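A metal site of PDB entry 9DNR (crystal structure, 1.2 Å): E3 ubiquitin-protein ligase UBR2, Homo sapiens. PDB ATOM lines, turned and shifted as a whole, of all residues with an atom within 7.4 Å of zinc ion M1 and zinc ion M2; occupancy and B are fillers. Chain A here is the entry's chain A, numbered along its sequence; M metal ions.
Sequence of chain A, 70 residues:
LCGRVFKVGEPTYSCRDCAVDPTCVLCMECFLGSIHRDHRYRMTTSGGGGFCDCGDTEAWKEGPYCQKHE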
ATOM      1  N   LEU A   1      -9.701  -2.732 -21.121  1.00  0.00           N
ATOM      2  CA  LEU A   1      -9.467  -4.167 -21.145  1.00  0.00           C
ATOM      3  C   LEU A   1      -9.787  -4.773 -22.509  1.00  0.00           C
ATOM      4  O   LEU A   1     -10.715  -4.350 -23.206  1.00  0.00           O
ATOM      5  CB  LEU A   1     -10.327  -4.874 -20.104  1.00  0.00           C
ATOM      6  CG  LEU A   1      -9.771  -5.069 -18.703  1.00  0.00           C
ATOM      7  CD1 LEU A   1      -9.683  -3.734 -17.987  1.00  0.00           C
ATOM      8  CD2 LEU A   1     -10.651  -6.040 -17.950  1.00  0.00           C
ATOM      9  N   CYS A   2      -9.011  -5.794 -22.871  1.00  0.00           N
ATOM     10  CA  CYS A   2      -9.242  -6.524 -24.111  1.00  0.00           C
ATOM     11  C   CYS A   2     -10.636  -7.148 -24.165  1.00  0.00           C
ATOM     12  O   CYS A   2     -11.467  -6.762 -24.991  1.00  0.00           O
ATOM     13  CB  CYS A   2      -8.193  -7.609 -24.305  1.00  0.00           C
ATOM     14  SG  CYS A   2      -8.497  -8.532 -25.818  1.00  0.00           S
ATOM     15  N   GLY A   3     -10.868  -8.136 -23.315  1.00  0.00           N
ATOM     16  CA  GLY A   3     -12.165  -8.757 -23.238  1.00  0.00           C
ATOM     17  C   GLY A   3     -12.585  -9.599 -24.421  1.00  0.00           C
ATOM     18  O   GLY A   3     -13.737 -10.064 -24.450  1.00  0.00           O
ATOM     19  N   ARG A   4     -11.705  -9.811 -25.409  1.00  0.00           N
ATOM     20  CA  ARG A   4     -12.096 -10.477 -26.653  1.00  0.00           C
ATOM     21  C   ARG A   4     -12.710 -11.845 -26.390  1.00  0.00           C
ATOM     22  O   ARG A   4     -12.132 -12.672 -25.694  1.00  0.00           O
ATOM     23  CB  ARG A   4     -10.893 -10.633 -27.593  1.00  0.00           C
ATOM     24  CG  ARG A   4     -11.289 -11.298 -28.899  1.00  0.00           C
ATOM     25  CD  ARG A   4     -10.130 -11.774 -29.754  1.00  0.00           C
ATOM     26  NE  ARG A   4      -9.227 -10.686 -30.126  1.00  0.00           N
ATOM     27  CZ  ARG A   4      -8.424 -10.725 -31.183  1.00  0.00           C
ATOM     28  NH1 ARG A   4      -8.438 -11.747 -32.023  1.00  0.00           N
ATOM     29  NH2 ARG A   4      -7.577  -9.726 -31.403  1.00  0.00           N
ATOM     30  N   PHE A   6     -13.484 -15.406 -27.880  1.00  0.00           N
ATOM     31  CA  PHE A   6     -12.900 -16.210 -28.946  1.00  0.00           C
ATOM     32  C   PHE A   6     -13.971 -16.753 -29.879  1.00  0.00           C
ATOM     33  O   PHE A   6     -15.075 -17.122 -29.453  1.00  0.00           O
ATOM     34  CB  PHE A   6     -12.142 -17.379 -28.357  1.00  0.00           C
ATOM     35  CG  PHE A   6     -11.057 -16.949 -27.463  1.00  0.00           C
ATOM     36  CD1 PHE A   6     -10.047 -16.114 -27.915  1.00  0.00           C
ATOM     37  CD2 PHE A   6     -11.045 -17.335 -26.133  1.00  0.00           C
ATOM     38  CE1 PHE A   6      -9.037 -15.695 -27.068  1.00  0.00           C
ATOM     39  CE2 PHE A   6     -10.037 -16.922 -25.299  1.00  0.00           C
ATOM     40  CZ  PHE A   6      -9.043 -16.112 -25.762  1.00  0.00           C
ATOM     41  N   VAL A  25      -5.875 -17.565 -20.446  1.00  0.00           N
ATOM     42  CA  VAL A  25      -5.539 -17.536 -21.861  1.00  0.00           C
ATOM     43  C   VAL A  25      -5.525 -16.105 -22.378  1.00  0.00           C
ATOM     44  O   VAL A  25      -6.141 -15.199 -21.813  1.00  0.00           O
ATOM     45  CB  VAL A  25      -6.540 -18.354 -22.698  1.00  0.00           C
ATOM     46  CG1 VAL A  25      -6.354 -19.852 -22.435  1.00  0.00           C
ATOM     47  CG2 VAL A  25      -7.970 -17.897 -22.400  1.00  0.00           C
ATOM     48  N   LEU A  26      -4.842 -15.928 -23.516  1.00  0.00           N
ATOM     49  CA  LEU A  26      -4.740 -14.649 -24.205  1.00  0.00           C
ATOM     50  C   LEU A  26      -5.127 -14.852 -25.650  1.00  0.00           C
ATOM     51  O   LEU A  26      -4.846 -15.901 -26.249  1.00  0.00           O
ATOM     52  CB  LEU A  26      -3.305 -14.121 -24.187  1.00  0.00           C
ATOM     53  CG  LEU A  26      -2.735 -13.802 -22.815  1.00  0.00           C
ATOM     54  CD1 LEU A  26      -1.255 -13.460 -22.926  1.00  0.00           C
ATOM     55  CD2 LEU A  26      -3.485 -12.660 -22.176  1.00  0.00           C
ATOM     56  N   CYS A  27      -5.761 -13.827 -26.235  1.00  0.00           N
ATOM     57  CA  CYS A  27      -5.967 -13.770 -27.680  1.00  0.00           C
ATOM     58  C   CYS A  27      -4.630 -13.515 -28.376  1.00  0.00           C
ATOM     59  O   CYS A  27      -3.612 -13.201 -27.750  1.00  0.00           O
ATOM     60  CB  CYS A  27      -6.957 -12.665 -28.026  1.00  0.00           C
ATOM     61  SG  CYS A  27      -6.315 -10.963 -27.877  1.00  0.00           S
ATOM     62  N   MET A  28      -4.628 -13.645 -29.695  1.00  0.00           N
ATOM     63  CA  MET A  28      -3.355 -13.564 -30.410  1.00  0.00           C
ATOM     64  C   MET A  28      -2.759 -12.172 -30.320  1.00  0.00           C
ATOM     65  O   MET A  28      -1.534 -12.032 -30.204  1.00  0.00           O
ATOM     66  CB  MET A  28      -3.516 -13.968 -31.872  1.00  0.00           C
ATOM     67  CG  MET A  28      -4.374 -13.047 -32.669  1.00  0.00           C
ATOM     68  SD  MET A  28      -4.531 -13.574 -34.365  1.00  0.00           S
ATOM     69  CE  MET A  28      -4.934 -15.287 -34.095  1.00  0.00           C
ATOM     70  N   GLU A  29      -3.589 -11.132 -30.344  1.00  0.00           N
ATOM     71  CA  GLU A  29      -3.037  -9.778 -30.293  1.00  0.00           C
ATOM     72  C   GLU A  29      -2.347  -9.532 -28.954  1.00  0.00           C
ATOM     73  O   GLU A  29      -1.233  -8.984 -28.900  1.00  0.00           O
ATOM     74  CB  GLU A  29      -4.190  -8.797 -30.519  1.00  0.00           C
ATOM     75  CG  GLU A  29      -3.830  -7.358 -30.315  1.00  0.00           C
ATOM     76  CD  GLU A  29      -5.042  -6.453 -30.379  1.00  0.00           C
ATOM     77  OE1 GLU A  29      -6.190  -6.948 -30.288  1.00  0.00           O
ATOM     78  OE2 GLU A  29      -4.824  -5.237 -30.526  1.00  0.00           O
ATOM     79  N   CYS A  30      -2.990  -9.955 -27.866  1.00  0.00           N
ATOM     80  CA  CYS A  30      -2.383  -9.743 -26.555  1.00  0.00           C
ATOM     81  C   CYS A  30      -1.156 -10.617 -26.352  1.00  0.00           C
ATOM     82  O   CYS A  30      -0.124 -10.151 -25.868  1.00  0.00           O
ATOM     83  CB  CYS A  30      -3.430  -9.933 -25.479  1.00  0.00           C
ATOM     84  SG  CYS A  30      -4.773  -8.709 -25.618  1.00  0.00           S
ATOM     85  N   PHE A  31      -1.240 -11.882 -26.759  1.00  0.00           N
ATOM     86  CA  PHE A  31      -0.097 -12.769 -26.631  1.00  0.00           C
ATOM     87  C   PHE A  31       1.134 -12.198 -27.351  1.00  0.00           C
ATOM     88  O   PHE A  31       2.223 -12.127 -26.780  1.00  0.00           O
ATOM     89  CB  PHE A  31      -0.448 -14.148 -27.170  1.00  0.00           C
ATOM     90  CG  PHE A  31       0.733 -15.027 -27.337  1.00  0.00           C
ATOM     91  CD1 PHE A  31       1.338 -15.570 -26.230  1.00  0.00           C
ATOM     92  CD2 PHE A  31       1.244 -15.313 -28.591  1.00  0.00           C
ATOM     93  CE1 PHE A  31       2.462 -16.386 -26.361  1.00  0.00           C
ATOM     94  CE2 PHE A  31       2.353 -16.141 -28.731  1.00  0.00           C
ATOM     95  CZ  PHE A  31       2.960 -16.669 -27.623  1.00  0.00           C
ATOM     96  N   GLY A  33       1.869  -9.210 -28.109  1.00  0.00           N
ATOM     97  CA  GLY A  33       2.348  -8.002 -27.471  1.00  0.00           C
ATOM     98  C   GLY A  33       2.700  -8.185 -26.008  1.00  0.00           C
ATOM     99  O   GLY A  33       2.853  -7.185 -25.293  1.00  0.00           O
ATOM    100  N   SER A  34       2.854  -9.414 -25.536  1.00  0.00           N
ATOM    101  CA  SER A  34       3.095  -9.680 -24.132  1.00  0.00           C
ATOM    102  C   SER A  34       4.495 -10.265 -23.933  1.00  0.00           C
ATOM    103  O   SER A  34       5.194 -10.656 -24.861  1.00  0.00           O
ATOM    104  CB  SER A  34       2.078 -10.686 -23.570  1.00  0.00           C
ATOM    105  OG  SER A  34       2.364 -12.018 -23.983  1.00  0.00           O
ATOM    106  N   PHE A  51     -12.913 -16.113 -23.208  1.00  0.00           N
ATOM    107  CA  PHE A  51     -12.476 -14.736 -23.428  1.00  0.00           C
ATOM    108  C   PHE A  51     -11.015 -14.560 -23.036  1.00  0.00           C
ATOM    109  O   PHE A  51     -10.470 -15.318 -22.218  1.00  0.00           O
ATOM    110  CB  PHE A  51     -13.362 -13.710 -22.722  1.00  0.00           C
ATOM    111  CG  PHE A  51     -13.453 -13.888 -21.240  1.00  0.00           C
ATOM    112  CD1 PHE A  51     -12.534 -13.259 -20.399  1.00  0.00           C
ATOM    113  CD2 PHE A  51     -14.427 -14.700 -20.672  1.00  0.00           C
ATOM    114  CE1 PHE A  51     -12.597 -13.436 -19.029  1.00  0.00           C
ATOM    115  CE2 PHE A  51     -14.491 -14.876 -19.302  1.00  0.00           C
ATOM    116  CZ  PHE A  51     -13.583 -14.236 -18.479  1.00  0.00           C
ATOM    117  N   CYS A  52     -10.413 -13.516 -23.596  1.00  0.00           N
ATOM    118  CA  CYS A  52      -9.039 -13.169 -23.301  1.00  0.00           C
ATOM    119  C   CYS A  52      -8.905 -12.618 -21.889  1.00  0.00           C
ATOM    120  O   CYS A  52      -9.696 -11.762 -21.457  1.00  0.00           O
ATOM    121  CB  CYS A  52      -8.572 -12.141 -24.322  1.00  0.00           C
ATOM    122  SG  CYS A  52      -6.890 -11.576 -24.044  1.00  0.00           S
ATOM    123  N   ASP A  53      -7.878 -13.088 -21.179  1.00  0.00           N
ATOM    124  CA  ASP A  53      -7.608 -12.699 -19.803  1.00  0.00           C
ATOM    125  C   ASP A  53      -6.550 -11.595 -19.678  1.00  0.00           C
ATOM    126  O   ASP A  53      -6.003 -11.405 -18.582  1.00  0.00           O
ATOM    127  CB  ASP A  53      -7.167 -13.901 -18.987  1.00  0.00           C
ATOM    128  CG  ASP A  53      -8.256 -14.933 -18.883  1.00  0.00           C
ATOM    129  OD1 ASP A  53      -9.398 -14.575 -18.513  1.00  0.00           O
ATOM    130  OD2 ASP A  53      -7.992 -16.097 -19.224  1.00  0.00           O
ATOM    131  N   CYS A  54      -6.266 -10.883 -20.759  1.00  0.00           N
ATOM    132  CA  CYS A  54      -5.319  -9.774 -20.645  1.00  0.00           C
ATOM    133  C   CYS A  54      -5.811  -8.772 -19.612  1.00  0.00           C
ATOM    134  O   CYS A  54      -6.970  -8.342 -19.641  1.00  0.00           O
ATOM    135  CB  CYS A  54      -5.135  -9.093 -22.001  1.00  0.00           C
ATOM    136  SG  CYS A  54      -4.067  -7.666 -21.934  1.00  0.00           S
ATOM    137  N   GLY A  55      -4.916  -8.417 -18.685  1.00  0.00           N
ATOM    138  CA  GLY A  55      -5.229  -7.483 -17.626  1.00  0.00           C
ATOM    139  C   GLY A  55      -5.572  -8.094 -16.285  1.00  0.00           C
ATOM    140  O   GLY A  55      -5.645  -7.358 -15.292  1.00  0.00           O
ATOM    141  N   PRO A  64       0.671  -9.483 -16.557  1.00  0.00           N
ATOM    142  CA  PRO A  64      -0.788  -9.606 -16.794  1.00  0.00           C
ATOM    143  C   PRO A  64      -1.303  -8.824 -17.981  1.00  0.00           C
ATOM    144  O   PRO A  64      -2.272  -9.268 -18.615  1.00  0.00           O
ATOM    145  CB  PRO A  64      -1.407  -9.109 -15.474  1.00  0.00           C
ATOM    146  CG  PRO A  64      -0.358  -8.187 -14.911  1.00  0.00           C
ATOM    147  CD  PRO A  64       0.961  -8.813 -15.270  1.00  0.00           C
ATOM    148  N   TYR A  65      -0.688  -7.713 -18.332  1.00  0.00           N
ATOM    149  CA  TYR A  65      -1.102  -6.875 -19.455  1.00  0.00           C
ATOM    150  C   TYR A  65      -0.122  -7.004 -20.615  1.00  0.00           C
ATOM    151  O   TYR A  65       1.076  -7.232 -20.406  1.00  0.00           O
ATOM    152  CB  TYR A  65      -1.138  -5.403 -19.049  1.00  0.00           C
ATOM    153  CG  TYR A  65      -2.303  -5.008 -18.175  1.00  0.00           C
ATOM    154  CD1 TYR A  65      -2.220  -5.081 -16.784  1.00  0.00           C
ATOM    155  CD2 TYR A  65      -3.483  -4.539 -18.734  1.00  0.00           C
ATOM    156  CE1 TYR A  65      -3.279  -4.687 -15.985  1.00  0.00           C
ATOM    157  CE2 TYR A  65      -4.554  -4.142 -17.943  1.00  0.00           C
ATOM    158  CZ  TYR A  65      -4.451  -4.223 -16.574  1.00  0.00           C
ATOM    159  OH  TYR A  65      -5.518  -3.840 -15.793  1.00  0.00           O
ATOM    160  N   CYS A  66      -0.636  -6.853 -21.826  1.00  0.00           N
ATOM    161  CA  CYS A  66       0.172  -6.719 -23.017  1.00  0.00           C
ATOM    162  C   CYS A  66       0.475  -5.246 -23.259  1.00  0.00           C
ATOM    163  O   CYS A  66      -0.040  -4.350 -22.573  1.00  0.00           O
ATOM    164  CB  CYS A  66      -0.547  -7.321 -24.228  1.00  0.00           C
ATOM    165  SG  CYS A  66      -1.866  -6.273 -24.861  1.00  0.00           S
ATOM    166  N   GLN A  67       1.303  -4.992 -24.271  1.00  0.00           N
ATOM    167  CA  GLN A  67       1.736  -3.626 -24.517  1.00  0.00           C
ATOM    168  C   GLN A  67       0.598  -2.718 -24.947  1.00  0.00           C
ATOM    169  O   GLN A  67       0.657  -1.500 -24.710  1.00  0.00           O
ATOM    170  CB  GLN A  67       2.886  -3.606 -25.522  1.00  0.00           C
ATOM    171  CG  GLN A  67       2.482  -3.842 -26.966  1.00  0.00           C
ATOM    172  CD  GLN A  67       3.649  -4.304 -27.828  1.00  0.00           C
ATOM    173  OE1 GLN A  67       4.762  -4.495 -27.329  1.00  0.00           O
ATOM    174  NE2 GLN A  67       3.415  -4.455 -29.129  1.00  0.00           N
ATOM    175  N   LYS A  68      -0.456  -3.273 -25.553  1.00  0.00           N
ATOM    176  CA  LYS A  68      -1.584  -2.470 -26.026  1.00  0.00           C
ATOM    177  C   LYS A  68      -2.504  -2.052 -24.894  1.00  0.00           C
ATOM    178  O   LYS A  68      -3.087  -0.957 -24.928  1.00  0.00           O
ATOM    179  CB  LYS A  68      -2.385  -3.278 -27.032  1.00  0.00           C
ATOM    180  CG  LYS A  68      -3.686  -2.607 -27.426  1.00  0.00           C
ATOM    181  CD  LYS A  68      -4.193  -3.172 -28.705  1.00  0.00           C
ATOM    182  CE  LYS A  68      -5.522  -2.551 -29.059  1.00  0.00           C
ATOM    183  NZ  LYS A  68      -5.994  -3.076 -30.351  1.00  0.00           N
ATOM    184  N   HIS A  69      -2.675  -2.903 -23.886  1.00  0.00           N
ATOM    185  CA  HIS A  69      -3.676  -2.653 -22.866  1.00  0.00           C
ATOM    186  C   HIS A  69      -3.088  -2.150 -21.550  1.00  0.00           C
ATOM    187  O   HIS A  69      -3.856  -1.680 -20.699  1.00  0.00           O
ATOM    188  CB  HIS A  69      -4.535  -3.908 -22.670  1.00  0.00           C
ATOM    189  CG  HIS A  69      -5.320  -4.253 -23.894  1.00  0.00           C
ATOM    190  ND1 HIS A  69      -5.122  -5.403 -24.617  1.00  0.00           N
ATOM    191  CD2 HIS A  69      -6.253  -3.536 -24.565  1.00  0.00           C
ATOM    192  CE1 HIS A  69      -5.948  -5.418 -25.648  1.00  0.00           C
ATOM    193  NE2 HIS A  69      -6.640  -4.288 -25.643  1.00  0.00           N
ATOM    194  N   GLU A  70      -1.775  -2.219 -21.384  1.00  0.00           N
ATOM    195  CA  GLU A  70      -1.101  -1.725 -20.168  1.00  0.00           C
ATOM    196  C   GLU A  70      -1.340  -0.226 -19.946  1.00  0.00           C
ATOM    197  O   GLU A  70      -1.317   0.223 -18.793  1.00  0.00           O
ATOM    198  CB  GLU A  70       0.420  -1.983 -20.206  1.00  0.00           C
ATOM    199  CG  GLU A  70       1.172  -1.204 -21.278  1.00  0.00           C
ATOM    200  CD  GLU A  70       2.646  -1.583 -21.383  1.00  0.00           C
ATOM    201  OE1 GLU A  70       3.175  -2.168 -20.418  1.00  0.00           O
ATOM    202  OE2 GLU A  70       3.283  -1.303 -22.418  1.00  0.00           O
ATOM    203  OXT GLU A  70      -1.517   0.544 -20.888  1.00  0.00           O
HETATM  204 ZN    ZN M   1      -6.748 -10.032 -25.797  1.00  0.00          ZN
HETATM  205 ZN    ZN M   2      -3.961  -7.046 -24.164  1.00  0.00          ZN
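Zinc ion M2 is bound by ND1 of His 69 (2.1 Å), SG of Cys 54 (2.3 Å), SG of Cys 66 (2.3 Å) and SG of Cys 30 (2.4 Å).
Zinc ion M2 has four donor atoms within binding distance.
Four residues have an atom within 4 Å of zinc ion M2: Cys 30, Cys 54, Cys 66 and His 69.
The nearest printed residue that does not touch zinc ion M2 is Cys 2 (4.3 Å).
N of Arg 4 lies close to SG of Cys 2, at 3.5 Å.
N of Cys 54 lies close to SG of Cys 52.
The side-chain sulfur (SG) of Cys 27 sits close to the guanidinium group (NE) of Arg 4 (3.7 Å).
The side-chain sulfur of Cys 27 sits close to the backbone NH of Glu 29 (3.7 Å).
The side-chain sulfur (SG) of Cys 66 lies close to the backbone NH (N) of Lys 68, at 3.4 Å.
The backbone carbonyl oxygen (O) of Arg 4 lies within hydrogen-bond range of the backbone NH (N) of Cys 52.
Four residues have an atom within 4 Å of zinc ion M1: Cys 2, Cys 27, Cys 30 and Cys 52.
Zinc ion M1 is bound by the side-chain sulfur (SG) of Cys 2 (2.3 Å), the side-chain sulfur (SG) of Cys 27 (2.3 Å), the side-chain sulfur (SG) of Cys 52 (2.3 Å) and the side-chain sulfur (SG) of Cys 30 (2.4 Å).
Zinc ion M1 has four donor atoms within binding distance.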
